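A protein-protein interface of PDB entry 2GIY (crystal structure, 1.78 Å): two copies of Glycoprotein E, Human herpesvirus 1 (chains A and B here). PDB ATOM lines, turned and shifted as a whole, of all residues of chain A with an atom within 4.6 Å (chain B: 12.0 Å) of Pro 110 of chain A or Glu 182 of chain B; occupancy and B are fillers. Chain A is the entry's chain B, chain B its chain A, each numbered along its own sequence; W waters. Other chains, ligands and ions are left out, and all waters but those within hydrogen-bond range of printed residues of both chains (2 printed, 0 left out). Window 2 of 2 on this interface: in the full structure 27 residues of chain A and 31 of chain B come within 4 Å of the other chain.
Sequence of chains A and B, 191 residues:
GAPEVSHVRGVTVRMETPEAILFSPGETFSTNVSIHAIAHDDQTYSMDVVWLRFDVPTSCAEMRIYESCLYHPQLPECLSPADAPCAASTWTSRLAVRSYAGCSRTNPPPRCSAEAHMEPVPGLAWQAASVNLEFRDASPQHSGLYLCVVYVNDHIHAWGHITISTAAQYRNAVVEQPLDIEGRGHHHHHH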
ATOM      1  N   PRO A 108     -17.899  -4.054 -33.352  1.00  0.00           N
ATOM      2  CA  PRO A 108     -18.453  -2.957 -32.546  1.00  0.00           C
ATOM      3  C   PRO A 108     -18.244  -1.547 -33.089  1.00  0.00           C
ATOM      4  O   PRO A 108     -17.164  -1.212 -33.579  1.00  0.00           O
ATOM      5  CB  PRO A 108     -17.774  -3.145 -31.193  1.00  0.00           C
ATOM      6  CG  PRO A 108     -17.550  -4.609 -31.133  1.00  0.00           C
ATOM      7  CD  PRO A 108     -17.037  -4.905 -32.514  1.00  0.00           C
ATOM      8  N   PRO A 109     -19.276  -0.692 -32.957  1.00  0.00           N
ATOM      9  CA  PRO A 109     -19.363   0.703 -33.387  1.00  0.00           C
ATOM     10  C   PRO A 109     -18.077   1.423 -33.749  1.00  0.00           C
ATOM     11  O   PRO A 109     -17.950   1.941 -34.860  1.00  0.00           O
ATOM     12  CB  PRO A 109     -20.120   1.348 -32.245  1.00  0.00           C
ATOM     13  CG  PRO A 109     -21.176   0.316 -32.002  1.00  0.00           C
ATOM     14  CD  PRO A 109     -20.422  -1.014 -32.086  1.00  0.00           C
ATOM     15  N   PRO A 110     -17.100   1.471 -32.832  1.00  0.00           N
ATOM     16  CA  PRO A 110     -15.883   2.181 -33.238  1.00  0.00           C
ATOM     17  C   PRO A 110     -15.351   1.686 -34.591  1.00  0.00           C
ATOM     18  O   PRO A 110     -15.144   2.462 -35.533  1.00  0.00           O
ATOM     19  CB  PRO A 110     -14.919   1.877 -32.093  1.00  0.00           C
ATOM     20  CG  PRO A 110     -15.828   1.765 -30.915  1.00  0.00           C
ATOM     21  CD  PRO A 110     -16.977   0.941 -31.463  1.00  0.00           C
ATOM     22  N   ARG A 111     -15.157   0.378 -34.679  1.00  0.00           N
ATOM     23  CA  ARG A 111     -14.622  -0.250 -35.880  1.00  0.00           C
ATOM     24  C   ARG A 111     -15.464  -0.075 -37.137  1.00  0.00           C
ATOM     25  O   ARG A 111     -14.925  -0.076 -38.245  1.00  0.00           O
ATOM     26  CB  ARG A 111     -14.420  -1.745 -35.630  1.00  0.00           C
ATOM     27  CG  ARG A 111     -13.652  -2.071 -34.362  1.00  0.00           C
ATOM     28  CD  ARG A 111     -13.579  -3.575 -34.142  1.00  0.00           C
ATOM     29  NE  ARG A 111     -12.838  -3.916 -32.931  1.00  0.00           N
ATOM     30  CZ  ARG A 111     -12.617  -5.158 -32.508  1.00  0.00           C
ATOM     31  NH1 ARG A 111     -13.083  -6.194 -33.196  1.00  0.00           N
ATOM     32  NH2 ARG A 111     -11.927  -5.364 -31.395  1.00  0.00           N
ATOM     33  N   CYS A 112     -16.776   0.063 -36.974  1.00  0.00           N
ATOM     34  CA  CYS A 112     -17.668   0.206 -38.124  1.00  0.00           C
ATOM     35  C   CYS A 112     -17.921   1.645 -38.565  1.00  0.00           C
ATOM     36  O   CYS A 112     -18.845   1.911 -39.333  1.00  0.00           O
ATOM     37  CB  CYS A 112     -18.997  -0.500 -37.841  1.00  0.00           C
ATOM     38  SG  CYS A 112     -19.826   0.050 -36.315  1.00  0.00           S
ATOM     39  N   SER A 113     -17.096   2.567 -38.081  1.00  0.00           N
ATOM     40  CA  SER A 113     -17.209   3.975 -38.452  1.00  0.00           C
ATOM     41  C   SER A 113     -17.178   4.048 -39.981  1.00  0.00           C
ATOM     42  O   SER A 113     -16.363   3.371 -40.617  1.00  0.00           O
ATOM     43  CB  SER A 113     -16.037   4.762 -37.862  1.00  0.00           C
ATOM     44  OG  SER A 113     -16.055   6.114 -38.281  1.00  0.00           O
ATOM     45  N   ALA A 129     -13.350  10.216 -34.841  1.00  0.00           N
ATOM     46  CA  ALA A 129     -14.100   9.076 -34.323  1.00  0.00           C
ATOM     47  C   ALA A 129     -14.910   9.373 -33.055  1.00  0.00           C
ATOM     48  O   ALA A 129     -15.353   8.450 -32.373  1.00  0.00           O
ATOM     49  CB  ALA A 129     -13.139   7.906 -34.071  1.00  0.00           C
ATOM     50  N   SER A 130     -15.114  10.650 -32.745  1.00  0.00           N
ATOM     51  CA  SER A 130     -15.870  11.032 -31.552  1.00  0.00           C
ATOM     52  C   SER A 130     -17.217  11.647 -31.913  1.00  0.00           C
ATOM     53  O   SER A 130     -17.369  12.237 -32.983  1.00  0.00           O
ATOM     54  CB  SER A 130     -15.071  12.033 -30.716  1.00  0.00           C
ATOM     55  OG  SER A 130     -15.829  12.503 -29.613  1.00  0.00           O
ATOM     56  N   VAL A 131     -18.195  11.501 -31.023  1.00  0.00           N
ATOM     57  CA  VAL A 131     -19.518  12.068 -31.267  1.00  0.00           C
ATOM     58  C   VAL A 131     -19.756  13.298 -30.401  1.00  0.00           C
ATOM     59  O   VAL A 131     -20.754  13.996 -30.562  1.00  0.00           O
ATOM     60  CB  VAL A 131     -20.649  11.034 -31.015  1.00  0.00           C
ATOM     61  CG1 VAL A 131     -20.604   9.951 -32.089  1.00  0.00           C
ATOM     62  CG2 VAL A 131     -20.520  10.423 -29.626  1.00  0.00           C
ATOM     63  N   ASN A 132     -18.837  13.568 -29.480  1.00  0.00           N
ATOM     64  CA  ASN A 132     -18.981  14.742 -28.629  1.00  0.00           C
ATOM     65  C   ASN A 132     -18.611  16.002 -29.396  1.00  0.00           C
ATOM     66  O   ASN A 132     -17.733  15.977 -30.255  1.00  0.00           O
ATOM     67  CB  ASN A 132     -18.114  14.602 -27.377  1.00  0.00           C
ATOM     68  CG  ASN A 132     -18.796  13.786 -26.301  1.00  0.00           C
ATOM     69  OD1 ASN A 132     -19.879  14.145 -25.838  1.00  0.00           O
ATOM     70  ND2 ASN A 132     -18.176  12.678 -25.904  1.00  0.00           N
ATOM     71  N   GLN B 177     -20.174  -1.410 -17.625  1.00  0.00           N
ATOM     72  CA  GLN B 177     -20.632  -1.446 -19.003  1.00  0.00           C
ATOM     73  C   GLN B 177     -19.529  -1.743 -20.007  1.00  0.00           C
ATOM     74  O   GLN B 177     -18.348  -1.517 -19.739  1.00  0.00           O
ATOM     75  CB  GLN B 177     -21.279  -0.097 -19.332  1.00  0.00           C
ATOM     76  CG  GLN B 177     -20.337   1.083 -19.110  1.00  0.00           C
ATOM     77  CD  GLN B 177     -21.025   2.294 -18.502  1.00  0.00           C
ATOM     78  OE1 GLN B 177     -21.988   2.824 -19.054  1.00  0.00           O
ATOM     79  NE2 GLN B 177     -20.524   2.742 -17.355  1.00  0.00           N
ATOM     80  N   PRO B 178     -19.901  -2.279 -21.180  1.00  0.00           N
ATOM     81  CA  PRO B 178     -18.877  -2.572 -22.184  1.00  0.00           C
ATOM     82  C   PRO B 178     -18.342  -1.228 -22.668  1.00  0.00           C
ATOM     83  O   PRO B 178     -18.879  -0.185 -22.291  1.00  0.00           O
ATOM     84  CB  PRO B 178     -19.659  -3.325 -23.258  1.00  0.00           C
ATOM     85  CG  PRO B 178     -21.025  -2.724 -23.159  1.00  0.00           C
ATOM     86  CD  PRO B 178     -21.242  -2.645 -21.668  1.00  0.00           C
ATOM     87  N   LEU B 179     -17.287  -1.237 -23.475  1.00  0.00           N
ATOM     88  CA  LEU B 179     -16.731   0.015 -23.971  1.00  0.00           C
ATOM     89  C   LEU B 179     -17.798   0.771 -24.754  1.00  0.00           C
ATOM     90  O   LEU B 179     -18.672   0.158 -25.366  1.00  0.00           O
ATOM     91  CB  LEU B 179     -15.519  -0.246 -24.867  1.00  0.00           C
ATOM     92  CG  LEU B 179     -14.283  -0.834 -24.179  1.00  0.00           C
ATOM     93  CD1 LEU B 179     -14.530  -2.293 -23.815  1.00  0.00           C
ATOM     94  CD2 LEU B 179     -13.091  -0.711 -25.113  1.00  0.00           C
ATOM     95  N   ASP B 180     -17.735   2.100 -24.723  1.00  0.00           N
ATOM     96  CA  ASP B 180     -18.714   2.904 -25.443  1.00  0.00           C
ATOM     97  C   ASP B 180     -18.447   2.876 -26.943  1.00  0.00           C
ATOM     98  O   ASP B 180     -17.511   2.221 -27.404  1.00  0.00           O
ATOM     99  CB  ASP B 180     -18.730   4.350 -24.935  1.00  0.00           C
ATOM    100  CG  ASP B 180     -17.390   5.041 -25.066  1.00  0.00           C
ATOM    101  OD1 ASP B 180     -16.602   4.680 -25.966  1.00  0.00           O
ATOM    102  OD2 ASP B 180     -17.138   5.971 -24.272  1.00  0.00           O
ATOM    103  N   ILE B 181     -19.272   3.584 -27.705  1.00  0.00           N
ATOM    104  CA  ILE B 181     -19.120   3.590 -29.153  1.00  0.00           C
ATOM    105  C   ILE B 181     -17.849   4.272 -29.642  1.00  0.00           C
ATOM    106  O   ILE B 181     -17.565   4.272 -30.841  1.00  0.00           O
ATOM    107  CB  ILE B 181     -20.340   4.232 -29.854  1.00  0.00           C
ATOM    108  CG1 ILE B 181     -20.440   5.716 -29.499  1.00  0.00           C
ATOM    109  CG2 ILE B 181     -21.606   3.484 -29.460  1.00  0.00           C
ATOM    110  CD1 ILE B 181     -21.584   6.425 -30.205  1.00  0.00           C
ATOM    111  N   GLU B 182     -17.089   4.860 -28.724  1.00  0.00           N
ATOM    112  CA  GLU B 182     -15.834   5.504 -29.098  1.00  0.00           C
ATOM    113  C   GLU B 182     -14.705   4.557 -28.697  1.00  0.00           C
ATOM    114  O   GLU B 182     -13.522   4.876 -28.830  1.00  0.00           O
ATOM    115  CB  GLU B 182     -15.687   6.865 -28.399  1.00  0.00           C
ATOM    116  CG  GLU B 182     -16.799   7.859 -28.749  1.00  0.00           C
ATOM    117  CD  GLU B 182     -16.567   9.248 -28.171  1.00  0.00           C
ATOM    118  OE1 GLU B 182     -15.683   9.396 -27.303  1.00  0.00           O
ATOM    119  OE2 GLU B 182     -17.276  10.194 -28.578  1.00  0.00           O
ATOM    120  N   GLY B 183     -15.096   3.380 -28.211  1.00  0.00           N
ATOM    121  CA  GLY B 183     -14.138   2.371 -27.796  1.00  0.00           C
ATOM    122  C   GLY B 183     -13.397   2.724 -26.521  1.00  0.00           C
ATOM    123  O   GLY B 183     -12.256   2.301 -26.325  1.00  0.00           O
ATOM    124  N   ARG B 184     -14.043   3.486 -25.644  1.00  0.00           N
ATOM    125  CA  ARG B 184     -13.417   3.899 -24.394  1.00  0.00           C
ATOM    126  C   ARG B 184     -14.252   3.532 -23.174  1.00  0.00           C
ATOM    127  O   ARG B 184     -15.373   4.012 -23.011  1.00  0.00           O
ATOM    128  CB  ARG B 184     -13.160   5.401 -24.416  1.00  0.00           C
ATOM    129  N   GLY B 185     -13.697   2.682 -22.316  1.00  0.00           N
ATOM    130  CA  GLY B 185     -14.402   2.278 -21.116  1.00  0.00           C
ATOM    131  C   GLY B 185     -13.506   2.291 -19.892  1.00  0.00           C
ATOM    132  O   GLY B 185     -13.577   1.339 -19.086  1.00  0.00           O
HETATM  133  O   HOH W   1     -17.203   6.227 -32.664  1.00  0.00           O
HETATM  134  O   HOH W   2     -15.670  11.917 -26.644  1.00  0.00           O
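Among the printed residues, merely in contact across the chains: Pro 109 of chain A with Ile 181 of chain B (3.8 Å), Pro 110 of chain A with Asp 180 of chain B (3.9 Å), Pro 110 of chain A with Glu 182 of chain B (3.7 Å), Pro 110 of chain A with Gly 183 of chain B (3.2 Å), Ala 129 of chain A with Glu 182 of chain B (3.9 Å) and Asn 132 of chain A with Glu 182 of chain B (3.8 Å).
No position is printed for both chains.
Of the 9 pairs that touch across the chains among the printed residues, none has its exchanged pair printed and touching as well.
The side-chain carboxylate (OD1) of Asp 180 of chain B sits at hydrogen-bond distance from the backbone NH (N) of Glu 182 of chain B (2.8 Å).
The side-chain carboxylate (OD1) of Asp 180 of chain B lies within hydrogen-bond range of the backbone NH (N) of Gly 183 of chain B, at 3.0 Å.
The backbone NH (N) of Arg 184 of chain B sits at hydrogen-bond distance from the side-chain carboxylate (OD1) of Asp 180 of chain B, 2.8 Å away.
The side-chain hydroxyl (OG) of Ser 130 of chain A sits at hydrogen-bond distance from the backbone NH (N) of Asn 132 of chain A, at 3.2 Å.
Of the printed residues of chain B, Pro 110 of chain A touches Asp 180, Ile 181, Glu 182 and Gly 183.
Of chain A, only Pro 110, Ala 129, Ser 130, Val 131 and Asn 132 come within 4 Å of Glu 182 of chain B.
No residue of chain B comes within 4 Å of Ser 113 of chain A.
Val 131 of chain A touches one residue of chain B.
Asn 132 of chain A touches just one residue of chain B: Glu 182.
Printed residues of chain A within 4 Å of Asp 180 of chain B: Pro 110 (3.9 Å).
Of the printed residues of chain A, Ile 181 of chain B touches Pro 109 (3.8 Å) and Pro 110 (3.1 Å).
Of the printed residues of chain A, Gly 183 of chain B touches Pro 110.
Arg 184 of chain B touches none of the printed residues of chain A.
Pro 178 of chain B touches none of the printed residues of chain A.
The nearest printed residue of chain A that does not touch Ile 181 of chain B is Val 131 of chain A (4.1 Å).
OE2 of Glu 182 of chain B lies within hydrogen-bond range of OG of Ser 130 of chain A (2.9 Å).
The side-chain carboxylate of Glu 182 of chain B sits at hydrogen-bond distance from the backbone NH of Val 131 of chain A, at 2.9 Å.
The backbone nitrogen of Pro 110 of chain A sits close to the backbone carbonyl oxygen of Ile 181 of chain B, at 3.5 Å.
Of the 10 printed residues of chain A, 6 touch a printed residue of chain B.
Of the 9 printed residues of chain B, 4 touch a printed residue of chain A.
Hydrophobic or aromatic side chains of chain B within 4 Å of the printed part of chain A: Ile 181.
Among the printed residues, no Asp or Glu carboxylate lies within 4 Å of a Lys or Arg side-chain nitrogen of the other chain.
Water W2 lies within hydrogen-bond range of OE1 of Glu 182 of chain B (2.6 Å), ND2 of Asn 132 of chain A (2.7 Å) and OG of Ser 130 of chain A (3.0 Å).
Water W1 bridges the backbone carbonyl oxygen of Ile 181 of chain B and the backbone carbonyl oxygen of Ala 129 of chain A.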
